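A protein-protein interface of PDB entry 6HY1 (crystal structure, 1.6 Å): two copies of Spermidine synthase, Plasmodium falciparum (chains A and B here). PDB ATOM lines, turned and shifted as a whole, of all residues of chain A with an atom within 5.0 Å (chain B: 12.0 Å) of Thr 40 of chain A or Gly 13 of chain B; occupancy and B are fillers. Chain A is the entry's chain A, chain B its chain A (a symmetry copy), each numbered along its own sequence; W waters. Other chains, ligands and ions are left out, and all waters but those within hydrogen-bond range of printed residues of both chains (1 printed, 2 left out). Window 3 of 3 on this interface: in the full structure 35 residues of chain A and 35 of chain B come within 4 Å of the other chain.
The backbone carbonyl oxygen (O) of Ala 15 of chain B is in hydrogen-bond range of the backbone NH (N) of Ser 17 of chain A (2.8 Å).
The backbone NH of Lys 19 of chain A is in hydrogen-bond range of the backbone carbonyl oxygen of Gly 13 of chain B, at 2.9 Å.
The side-chain hydroxyl of Thr 41 of chain A sits at hydrogen-bond distance from the backbone carbonyl oxygen of Pro 12 of chain B (3.2 Å).
The side-chain amide oxygen (OE1) of Gln 14 of chain B sits at hydrogen-bond distance from the side-chain hydroxyl (OH) of Tyr 42 of chain A.
The side-chain sulfur (SG) of Cys 226 of chain B sits at hydrogen-bond distance from the side-chain hydroxyl (OH) of Tyr 42 of chain A.
Of the printed residues of chain B, Trp 3 of chain A touches Phe 7, Gly 13, Gln 14 and Ala 15.
Of chain B, only Gln 14 and Ala 15 come within 4 Å of Ser 17 of chain A.
Of chain B, only Gly 13 (3.5 Å) comes within 4 Å of Leu 18 of chain A.
Of chain B, only Gly 13 (2.9 Å) comes within 4 Å of Lys 19 of chain A.
No residue of chain B comes within 4 Å of Ser 39 of chain A.
Of chain B, only Gly 13 comes within 4 Å of Thr 40 of chain A.
Thr 41 of chain A touches just these residues of chain B: Pro 12 (3.2 Å) and Gly 13 (3.8 Å).
Of chain B, only Gln 14 (2.7 Å) and Cys 226 (3.4 Å) come within 4 Å of Tyr 42 of chain A.
Printed residues of chain A within 4 Å of Phe 7 of chain B: Trp 3 (3.6 Å).
Trp 11 of chain B touches none of the printed residues of chain A.
Of the printed residues of chain A, Pro 12 of chain B touches Thr 41 (3.2 Å).
Printed residues of chain A within 4 Å of Ala 15 of chain B: Trp 3 (3.9 Å) and Ser 17 (2.8 Å).
His 196 of chain B touches none of the printed residues of chain A.
Of the printed residues of chain A, Cys 226 of chain B touches Tyr 42 (3.4 Å).
The nearest residue of chain B that does not touch Thr 40 of chain A is Pro 12 of chain B (5.2 Å).
The nearest printed residue of chain A that does not touch Cys 226 of chain B is Leu 18 of chain A (8.5 Å).
Water W1 lies within hydrogen-bond range of O of Gly 13 of chain B (2.9 Å), OG1 of Thr 41 of chain A (2.9 Å), OG1 of Thr 40 of chain A (3.2 Å) and O of Lys 19 of chain A (3.5 Å).
Of the 19 printed residues of chain B, 6 touch a printed residue of chain A.
Printed residues of chain B that touch a printed residue of chain A: Phe 7, Pro 12, Gly 13, Gln 14, Ala 15 and Cys 226.
Hydrophobic or aromatic side chains of chain B that line the printed part of chain A: Phe 7.
Hydrophobic or aromatic side chains of chain A within 4 Å of the printed part of chain B: Trp 3, Leu 18 and Tyr 42.
Along chain A the printed residues that touch a printed residue of chain B span positions 3 to 42.
Among the printed residues, no Asp or Glu carboxylate lies within 4 Å of a Lys or Arg side-chain nitrogen of the other chain.
Among the printed residues, merely in contact across the chains: Trp 3 of chain A with Phe 7 of chain B, Trp 3 of chain A with Gly 13 of chain B, Trp 3 of chain A with Gln 14 of chain B, Trp 3 of chain A with Ala 15 of chain B, Ser 17 of chain A with Gln 14 of chain B, Leu 18 of chain A with Gly 13 of chain B, Thr 40 of chain A with Gly 13 of chain B and Thr 41 of chain A with Gly 13 of chain B.
1 position is printed for both chains.
O of Lys 19 of chain A is in hydrogen-bond range of N of Thr 40 of chain A (3.0 Å).
The side-chain hydroxyl (OG) of Ser 39 of chain A is in hydrogen-bond range of the backbone NH (N) of Tyr 42 of chain A, at 2.8 Å.
NE2 of Gln 14 of chain B sits at hydrogen-bond distance from SG of Cys 226 of chain B (3.5 Å).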
ATOM      1  N   LYS A   1      -7.497   4.775  20.716  1.00  0.00           N
ATOM      2  CA  LYS A   1      -7.493   5.353  22.064  1.00  0.00           C
ATOM      3  C   LYS A   1      -8.770   6.158  22.333  1.00  0.00           C
ATOM      4  O   LYS A   1      -9.209   6.919  21.476  1.00  0.00           O
ATOM      5  CB  LYS A   1      -6.260   6.247  22.274  1.00  0.00           C
ATOM      6  CG  LYS A   1      -4.955   5.479  22.452  1.00  0.00           C
ATOM      7  CD  LYS A   1      -3.857   6.362  23.022  1.00  0.00           C
ATOM      8  CE  LYS A   1      -2.535   5.620  23.050  1.00  0.00           C
ATOM      9  NZ  LYS A   1      -2.218   5.094  21.686  1.00  0.00           N
ATOM     10  N   TRP A   3     -11.195   8.877  24.816  1.00  0.00           N
ATOM     11  CA  TRP A   3     -11.047  10.158  25.509  1.00  0.00           C
ATOM     12  C   TRP A   3     -11.942  10.183  26.742  1.00  0.00           C
ATOM     13  O   TRP A   3     -13.073   9.669  26.715  1.00  0.00           O
ATOM     14  CB  TRP A   3     -11.434  11.344  24.574  1.00  0.00           C
ATOM     15  CG  TRP A   3     -10.455  11.587  23.467  1.00  0.00           C
ATOM     16  CD1 TRP A   3     -10.283  10.827  22.334  1.00  0.00           C
ATOM     17  CD2 TRP A   3      -9.552  12.694  23.343  1.00  0.00           C
ATOM     18  NE1 TRP A   3      -9.295  11.373  21.540  1.00  0.00           N
ATOM     19  CE2 TRP A   3      -8.842  12.530  22.129  1.00  0.00           C
ATOM     20  CE3 TRP A   3      -9.253  13.795  24.157  1.00  0.00           C
ATOM     21  CZ2 TRP A   3      -7.857  13.432  21.705  1.00  0.00           C
ATOM     22  CZ3 TRP A   3      -8.277  14.701  23.729  1.00  0.00           C
ATOM     23  CH2 TRP A   3      -7.585  14.505  22.522  1.00  0.00           C
ATOM     24  N   SER A  17     -11.502  17.679  27.685  1.00  0.00           N
ATOM     25  CA  SER A  17     -11.268  16.255  27.445  1.00  0.00           C
ATOM     26  C   SER A  17      -9.786  15.940  27.438  1.00  0.00           C
ATOM     27  O   SER A  17      -8.960  16.752  27.018  1.00  0.00           O
ATOM     28  CB  SER A  17     -11.877  15.812  26.098  1.00  0.00           C
ATOM     29  OG  SER A  17     -13.277  16.035  26.056  1.00  0.00           O
ATOM     30  N   LEU A  18      -9.447  14.731  27.919  1.00  0.00           N
ATOM     31  CA  LEU A  18      -8.077  14.234  27.988  1.00  0.00           C
ATOM     32  C   LEU A  18      -8.060  12.875  27.308  1.00  0.00           C
ATOM     33  O   LEU A  18      -8.916  12.030  27.596  1.00  0.00           O
ATOM     34  CB  LEU A  18      -7.566  14.044  29.419  1.00  0.00           C
ATOM     35  CG  LEU A  18      -7.274  15.354  30.140  1.00  0.00           C
ATOM     36  CD1 LEU A  18      -6.974  15.015  31.616  1.00  0.00           C
ATOM     37  CD2 LEU A  18      -6.069  16.059  29.498  1.00  0.00           C
ATOM     38  N   LYS A  19      -7.073  12.662  26.445  1.00  0.00           N
ATOM     39  CA  LYS A  19      -6.927  11.371  25.801  1.00  0.00           C
ATOM     40  C   LYS A  19      -6.448  10.344  26.825  1.00  0.00           C
ATOM     41  O   LYS A  19      -5.572  10.631  27.649  1.00  0.00           O
ATOM     42  CB  LYS A  19      -5.940  11.474  24.635  1.00  0.00           C
ATOM     43  CG  LYS A  19      -6.080  10.302  23.637  1.00  0.00           C
ATOM     44  CD  LYS A  19      -5.113  10.440  22.462  1.00  0.00           C
ATOM     45  CE  LYS A  19      -5.271   9.215  21.531  1.00  0.00           C
ATOM     46  NZ  LYS A  19      -4.217   9.065  20.474  1.00  0.00           N
ATOM     47  N   ILE A  20      -7.036   9.139  26.768  1.00  0.00           N
ATOM     48  CA  ILE A  20      -6.751   8.062  27.731  1.00  0.00           C
ATOM     49  C   ILE A  20      -5.682   7.142  27.159  1.00  0.00           C
ATOM     50  O   ILE A  20      -5.904   6.510  26.112  1.00  0.00           O
ATOM     51  CB  ILE A  20      -8.010   7.245  28.060  1.00  0.00           C
ATOM     52  CG1 ILE A  20      -9.086   8.106  28.733  1.00  0.00           C
ATOM     53  CG2 ILE A  20      -7.624   6.020  28.960  1.00  0.00           C
ATOM     54  CD1 ILE A  20     -10.497   7.569  28.591  1.00  0.00           C
ATOM     55  N   LYS A  21      -4.544   7.042  27.855  1.00  0.00           N
ATOM     56  CA  LYS A  21      -3.562   5.995  27.560  1.00  0.00           C
ATOM     57  C   LYS A  21      -4.018   4.644  28.113  1.00  0.00           C
ATOM     58  O   LYS A  21      -4.093   3.659  27.366  1.00  0.00           O
ATOM     59  CB  LYS A  21      -2.188   6.362  28.110  1.00  0.00           C
ATOM     60  CG  LYS A  21      -1.095   5.411  27.639  1.00  0.00           C
ATOM     61  CD  LYS A  21       0.226   5.766  28.263  1.00  0.00           C
ATOM     62  CE  LYS A  21       1.352   4.929  27.687  1.00  0.00           C
ATOM     63  NZ  LYS A  21       2.660   5.345  28.262  1.00  0.00           N
ATOM     64  N   GLU A  38      -4.335   6.764  33.315  1.00  0.00           N
ATOM     65  CA  GLU A  38      -3.153   7.423  32.787  1.00  0.00           C
ATOM     66  C   GLU A  38      -3.554   8.144  31.507  1.00  0.00           C
ATOM     67  O   GLU A  38      -4.001   7.511  30.553  1.00  0.00           O
ATOM     68  CB  GLU A  38      -2.035   6.424  32.496  1.00  0.00           C
ATOM     69  CG  GLU A  38      -0.743   7.140  32.162  1.00  0.00           C
ATOM     70  CD  GLU A  38       0.391   6.215  31.849  1.00  0.00           C
ATOM     71  OE1 GLU A  38       1.533   6.710  31.743  1.00  0.00           O
ATOM     72  OE2 GLU A  38       0.152   4.994  31.709  1.00  0.00           O
ATOM     73  N   SER A  39      -3.414   9.466  31.498  1.00  0.00           N
ATOM     74  CA  SER A  39      -3.653  10.224  30.286  1.00  0.00           C
ATOM     75  C   SER A  39      -2.418  10.153  29.381  1.00  0.00           C
ATOM     76  O   SER A  39      -1.330   9.761  29.805  1.00  0.00           O
ATOM     77  CB  SER A  39      -3.988  11.682  30.652  1.00  0.00           C
ATOM     78  OG  SER A  39      -2.818  12.377  31.066  1.00  0.00           O
ATOM     79  N   THR A  40      -2.569  10.570  28.120  1.00  0.00           N
ATOM     80  CA  THR A  40      -1.402  10.565  27.234  1.00  0.00           C
ATOM     81  C   THR A  40      -0.442  11.729  27.482  1.00  0.00           C
ATOM     82  O   THR A  40       0.756  11.600  27.215  1.00  0.00           O
ATOM     83  CB  THR A  40      -1.839  10.566  25.757  1.00  0.00           C
ATOM     84  OG1 THR A  40      -2.651  11.707  25.480  1.00  0.00           O
ATOM     85  CG2 THR A  40      -2.645   9.332  25.430  1.00  0.00           C
ATOM     86  N   THR A  41      -0.916  12.876  27.970  1.00  0.00           N
ATOM     87  CA  THR A  41      -0.025  14.022  28.096  1.00  0.00           C
ATOM     88  C   THR A  41      -0.074  14.710  29.458  1.00  0.00           C
ATOM     89  O   THR A  41       0.795  15.543  29.729  1.00  0.00           O
ATOM     90  CB  THR A  41      -0.303  15.045  26.978  1.00  0.00           C
ATOM     91  OG1 THR A  41      -1.663  15.444  27.025  1.00  0.00           O
ATOM     92  CG2 THR A  41      -0.069  14.415  25.616  1.00  0.00           C
ATOM     93  N   TYR A  42      -1.026  14.381  30.333  1.00  0.00           N
ATOM     94  CA  TYR A  42      -1.083  14.989  31.658  1.00  0.00           C
ATOM     95  C   TYR A  42      -0.734  14.009  32.784  1.00  0.00           C
ATOM     96  O   TYR A  42      -0.943  14.329  33.967  1.00  0.00           O
ATOM     97  CB  TYR A  42      -2.463  15.614  31.893  1.00  0.00           C
ATOM     98  CG  TYR A  42      -2.595  16.978  31.236  1.00  0.00           C
ATOM     99  CD1 TYR A  42      -2.766  17.085  29.867  1.00  0.00           C
ATOM    100  CD2 TYR A  42      -2.487  18.137  31.985  1.00  0.00           C
ATOM    101  CE1 TYR A  42      -2.882  18.342  29.250  1.00  0.00           C
ATOM    102  CE2 TYR A  42      -2.586  19.401  31.377  1.00  0.00           C
ATOM    103  CZ  TYR A  42      -2.785  19.464  30.012  1.00  0.00           C
ATOM    104  OH  TYR A  42      -2.877  20.690  29.402  1.00  0.00           O
ATOM    105  N   SER B   5     -15.503  20.889  18.918  1.00  0.00           N
ATOM    106  CA  SER B   5     -14.339  20.447  19.701  1.00  0.00           C
ATOM    107  C   SER B   5     -13.038  20.942  19.087  1.00  0.00           C
ATOM    108  O   SER B   5     -12.810  20.789  17.883  1.00  0.00           O
ATOM    109  CB  SER B   5     -14.289  18.904  19.820  1.00  0.00           C
ATOM    110  OG  SER B   5     -15.401  18.455  20.573  1.00  0.00           O
ATOM    111  N   GLU B   6     -12.175  21.531  19.919  1.00  0.00           N
ATOM    112  CA  GLU B   6     -10.914  22.116  19.456  1.00  0.00           C
ATOM    113  C   GLU B   6      -9.790  21.105  19.684  1.00  0.00           C
ATOM    114  O   GLU B   6      -9.226  21.043  20.768  1.00  0.00           O
ATOM    115  CB  GLU B   6     -10.615  23.403  20.216  1.00  0.00           C
ATOM    116  CG  GLU B   6      -9.460  24.225  19.637  1.00  0.00           C
ATOM    117  CD  GLU B   6      -9.060  25.366  20.546  1.00  0.00           C
ATOM    118  OE1 GLU B   6      -8.834  25.100  21.752  1.00  0.00           O
ATOM    119  OE2 GLU B   6      -8.947  26.537  20.070  1.00  0.00           O
ATOM    120  N   PHE B   7      -9.452  20.327  18.654  1.00  0.00           N
ATOM    121  CA  PHE B   7      -8.332  19.393  18.670  1.00  0.00           C
ATOM    122  C   PHE B   7      -7.174  19.984  17.875  1.00  0.00           C
ATOM    123  O   PHE B   7      -7.391  20.633  16.854  1.00  0.00           O
ATOM    124  CB  PHE B   7      -8.692  18.038  18.031  1.00  0.00           C
ATOM    125  CG  PHE B   7      -9.758  17.260  18.749  1.00  0.00           C
ATOM    126  CD1 PHE B   7      -9.427  16.378  19.769  1.00  0.00           C
ATOM    127  CD2 PHE B   7     -11.084  17.369  18.370  1.00  0.00           C
ATOM    128  CE1 PHE B   7     -10.407  15.635  20.428  1.00  0.00           C
ATOM    129  CE2 PHE B   7     -12.069  16.626  19.017  1.00  0.00           C
ATOM    130  CZ  PHE B   7     -11.732  15.772  20.053  1.00  0.00           C
ATOM    131  N   SER B   8      -5.939  19.731  18.312  1.00  0.00           N
ATOM    132  CA  SER B   8      -4.820  20.244  17.526  1.00  0.00           C
ATOM    133  C   SER B   8      -3.544  19.489  17.863  1.00  0.00           C
ATOM    134  O   SER B   8      -3.316  19.138  19.019  1.00  0.00           O
ATOM    135  CB  SER B   8      -4.623  21.756  17.779  1.00  0.00           C
ATOM    136  OG  SER B   8      -3.487  22.274  17.097  1.00  0.00           O
ATOM    137  N   ILE B   9      -2.706  19.253  16.850  1.00  0.00           N
ATOM    138  CA  ILE B   9      -1.357  18.768  17.121  1.00  0.00           C
ATOM    139  C   ILE B   9      -0.557  19.767  17.956  1.00  0.00           C
ATOM    140  O   ILE B   9       0.489  19.413  18.530  1.00  0.00           O
ATOM    141  CB  ILE B   9      -0.628  18.461  15.799  1.00  0.00           C
ATOM    142  CG1 ILE B   9      -0.519  19.750  14.972  1.00  0.00           C
ATOM    143  CG2 ILE B   9      -1.341  17.338  15.031  1.00  0.00           C
ATOM    144  CD1 ILE B   9       0.009  19.556  13.564  1.00  0.00           C
ATOM    145  N   MET B  10      -1.021  21.019  18.039  1.00  0.00           N
ATOM    146  CA  MET B  10      -0.325  22.022  18.833  1.00  0.00           C
ATOM    147  C   MET B  10      -0.527  21.824  20.334  1.00  0.00           C
ATOM    148  O   MET B  10       0.245  22.366  21.133  1.00  0.00           O
ATOM    149  CB  MET B  10      -0.787  23.421  18.401  1.00  0.00           C
ATOM    150  CG  MET B  10      -0.315  23.766  16.996  1.00  0.00           C
ATOM    151  SD  MET B  10      -0.770  25.445  16.428  1.00  0.00           S
ATOM    152  CE  MET B  10      -2.572  25.338  16.355  1.00  0.00           C
ATOM    153  N   TRP B  11      -1.556  21.077  20.733  1.00  0.00           N
ATOM    154  CA  TRP B  11      -1.795  20.725  22.133  1.00  0.00           C
ATOM    155  C   TRP B  11      -2.310  19.290  22.152  1.00  0.00           C
ATOM    156  O   TRP B  11      -3.486  19.034  22.428  1.00  0.00           O
ATOM    157  CB  TRP B  11      -2.781  21.689  22.799  1.00  0.00           C
ATOM    158  CG  TRP B  11      -3.918  22.227  21.966  1.00  0.00           C
ATOM    159  CD1 TRP B  11      -5.158  21.687  21.827  1.00  0.00           C
ATOM    160  CD2 TRP B  11      -3.918  23.447  21.202  1.00  0.00           C
ATOM    161  NE1 TRP B  11      -5.938  22.483  21.003  1.00  0.00           N
ATOM    162  CE2 TRP B  11      -5.197  23.574  20.616  1.00  0.00           C
ATOM    163  CE3 TRP B  11      -2.954  24.419  20.942  1.00  0.00           C
ATOM    164  CZ2 TRP B  11      -5.539  24.647  19.776  1.00  0.00           C
ATOM    165  CZ3 TRP B  11      -3.295  25.504  20.117  1.00  0.00           C
ATOM    166  CH2 TRP B  11      -4.576  25.600  19.545  1.00  0.00           C
ATOM    167  N   PRO B  12      -1.454  18.331  21.829  1.00  0.00           N
ATOM    168  CA  PRO B  12      -1.917  16.938  21.714  1.00  0.00           C
ATOM    169  C   PRO B  12      -2.482  16.400  23.024  1.00  0.00           C
ATOM    170  O   PRO B  12      -2.012  16.729  24.112  1.00  0.00           O
ATOM    171  CB  PRO B  12      -0.644  16.181  21.317  1.00  0.00           C
ATOM    172  CG  PRO B  12       0.462  16.981  21.943  1.00  0.00           C
ATOM    173  CD  PRO B  12       0.021  18.433  21.861  1.00  0.00           C
ATOM    174  N   GLY B  13      -3.494  15.531  22.906  1.00  0.00           N
ATOM    175  CA  GLY B  13      -3.983  14.828  24.069  1.00  0.00           C
ATOM    176  C   GLY B  13      -4.995  15.561  24.907  1.00  0.00           C
ATOM    177  O   GLY B  13      -5.420  15.020  25.932  1.00  0.00           O
ATOM    178  N   GLN B  14      -5.388  16.784  24.534  1.00  0.00           N
ATOM    179  CA  GLN B  14      -6.381  17.525  25.288  1.00  0.00           C
ATOM    180  C   GLN B  14      -7.305  18.186  24.282  1.00  0.00           C
ATOM    181  O   GLN B  14      -6.933  18.380  23.128  1.00  0.00           O
ATOM    182  CB  GLN B  14      -5.743  18.604  26.187  1.00  0.00           C
ATOM    183  CG  GLN B  14      -5.174  19.758  25.386  1.00  0.00           C
ATOM    184  CD  GLN B  14      -4.405  20.732  26.243  1.00  0.00           C
ATOM    185  OE1 GLN B  14      -3.300  20.408  26.719  1.00  0.00           O
ATOM    186  NE2 GLN B  14      -4.965  21.936  26.445  1.00  0.00           N
ATOM    187  N   ALA B  15      -8.511  18.512  24.722  1.00  0.00           N
ATOM    188  CA  ALA B  15      -9.417  19.241  23.841  1.00  0.00           C
ATOM    189  C   ALA B  15     -10.449  19.981  24.675  1.00  0.00           C
ATOM    190  O   ALA B  15     -10.853  19.514  25.739  1.00  0.00           O
ATOM    191  CB  ALA B  15     -10.126  18.278  22.856  1.00  0.00           C
ATOM    192  N   PHE B  16     -10.886  21.143  24.194  1.00  0.00           N
ATOM    193  CA  PHE B  16     -11.935  21.903  24.849  1.00  0.00           C
ATOM    194  C   PHE B  16     -13.112  21.917  23.891  1.00  0.00           C
ATOM    195  O   PHE B  16     -12.903  21.996  22.685  1.00  0.00           O
ATOM    196  CB  PHE B  16     -11.447  23.355  25.155  1.00  0.00           C
ATOM    197  CG  PHE B  16     -12.486  24.242  25.734  1.00  0.00           C
ATOM    198  CD1 PHE B  16     -12.973  24.034  27.001  1.00  0.00           C
ATOM    199  CD2 PHE B  16     -12.989  25.319  24.996  1.00  0.00           C
ATOM    200  CE1 PHE B  16     -13.925  24.862  27.544  1.00  0.00           C
ATOM    201  CE2 PHE B  16     -13.946  26.171  25.534  1.00  0.00           C
ATOM    202  CZ  PHE B  16     -14.426  25.952  26.792  1.00  0.00           C
ATOM    203  N   SER B  17     -14.338  21.819  24.417  1.00  0.00           N
ATOM    204  CA  SER B  17     -15.539  21.735  23.586  1.00  0.00           C
ATOM    205  C   SER B  17     -16.599  22.708  24.060  1.00  0.00           C
ATOM    206  O   SER B  17     -16.727  22.985  25.254  1.00  0.00           O
ATOM    207  CB  SER B  17     -16.128  20.309  23.604  1.00  0.00           C
ATOM    208  OG  SER B  17     -15.200  19.351  23.124  1.00  0.00           O
ATOM    209  N   GLU B 191       3.045  31.653  23.345  1.00  0.00           N
ATOM    210  CA  GLU B 191       2.508  30.338  23.736  1.00  0.00           C
ATOM    211  C   GLU B 191       2.051  30.301  25.205  1.00  0.00           C
ATOM    212  O   GLU B 191       2.625  30.965  26.080  1.00  0.00           O
ATOM    213  CB  GLU B 191       3.559  29.240  23.477  1.00  0.00           C
ATOM    214  CG  GLU B 191       3.299  27.812  24.146  1.00  0.00           C
ATOM    215  CD  GLU B 191       2.259  26.919  23.431  1.00  0.00           C
ATOM    216  OE1 GLU B 191       2.601  25.746  23.116  1.00  0.00           O
ATOM    217  OE2 GLU B 191       1.102  27.370  23.202  1.00  0.00           O
ATOM    218  N   TRP B 194       1.530  26.613  30.028  1.00  0.00           N
ATOM    219  CA  TRP B 194       1.270  25.207  30.357  1.00  0.00           C
ATOM    220  C   TRP B 194       1.531  24.252  29.206  1.00  0.00           C
ATOM    221  O   TRP B 194       1.456  23.037  29.412  1.00  0.00           O
ATOM    222  CB  TRP B 194      -0.174  25.000  30.814  1.00  0.00           C
ATOM    223  CG  TRP B 194      -0.415  25.547  32.139  1.00  0.00           C
ATOM    224  CD1 TRP B 194      -1.092  26.681  32.466  1.00  0.00           C
ATOM    225  CD2 TRP B 194       0.046  24.976  33.376  1.00  0.00           C
ATOM    226  NE1 TRP B 194      -1.111  26.849  33.835  1.00  0.00           N
ATOM    227  CE2 TRP B 194      -0.412  25.814  34.415  1.00  0.00           C
ATOM    228  CE3 TRP B 194       0.765  23.813  33.691  1.00  0.00           C
ATOM    229  CZ2 TRP B 194      -0.135  25.565  35.775  1.00  0.00           C
ATOM    230  CZ3 TRP B 194       1.053  23.550  35.064  1.00  0.00           C
ATOM    231  CH2 TRP B 194       0.578  24.412  36.076  1.00  0.00           C
ATOM    232  N   ILE B 195       1.857  24.744  28.015  1.00  0.00           N
ATOM    233  CA  ILE B 195       2.070  23.844  26.883  1.00  0.00           C
ATOM    234  C   ILE B 195       3.527  23.831  26.461  1.00  0.00           C
ATOM    235  O   ILE B 195       4.350  23.154  27.088  1.00  0.00           O
ATOM    236  CB  ILE B 195       1.155  24.224  25.704  1.00  0.00           C
ATOM    237  CG1 ILE B 195      -0.244  24.493  26.224  1.00  0.00           C
ATOM    238  CG2 ILE B 195       1.127  23.107  24.704  1.00  0.00           C
ATOM    239  CD1 ILE B 195      -1.285  24.674  25.098  1.00  0.00           C
ATOM    240  N   HIS B 196       3.885  24.595  25.431  1.00  0.00           N
ATOM    241  CA  HIS B 196       5.251  24.503  24.900  1.00  0.00           C
ATOM    242  C   HIS B 196       6.072  25.693  25.418  1.00  0.00           C
ATOM    243  O   HIS B 196       6.118  26.785  24.837  1.00  0.00           O
ATOM    244  CB  HIS B 196       5.226  24.345  23.383  1.00  0.00           C
ATOM    245  CG  HIS B 196       4.540  23.079  22.940  1.00  0.00           C
ATOM    246  ND1 HIS B 196       3.735  23.009  21.819  1.00  0.00           N
ATOM    247  CD2 HIS B 196       4.520  21.837  23.491  1.00  0.00           C
ATOM    248  CE1 HIS B 196       3.253  21.782  21.698  1.00  0.00           C
ATOM    249  NE2 HIS B 196       3.712  21.051  22.700  1.00  0.00           N
ATOM    250  N   PRO B 225      -6.507  27.331  24.740  1.00  0.00           N
ATOM    251  CA  PRO B 225      -6.088  26.047  25.339  1.00  0.00           C
ATOM    252  C   PRO B 225      -5.287  26.274  26.617  1.00  0.00           C
ATOM    253  O   PRO B 225      -4.421  27.158  26.687  1.00  0.00           O
ATOM    254  CB  PRO B 225      -5.210  25.407  24.264  1.00  0.00           C
ATOM    255  CG  PRO B 225      -5.499  26.173  22.969  1.00  0.00           C
ATOM    256  CD  PRO B 225      -6.058  27.492  23.345  1.00  0.00           C
ATOM    257  N   CYS B 226      -5.574  25.435  27.621  1.00  0.00           N
ATOM    258  CA  CYS B 226      -5.035  25.526  28.979  1.00  0.00           C
ATOM    259  C   CYS B 226      -5.541  26.742  29.760  1.00  0.00           C
ATOM    260  O   CYS B 226      -5.095  26.984  30.906  1.00  0.00           O
ATOM    261  CB  CYS B 226      -3.499  25.488  28.975  1.00  0.00           C
ATOM    262  SG  CYS B 226      -2.850  23.893  28.402  1.00  0.00           S
HETATM  263  O   HOH W   1      -3.786  13.586  27.820  1.00  0.00           O
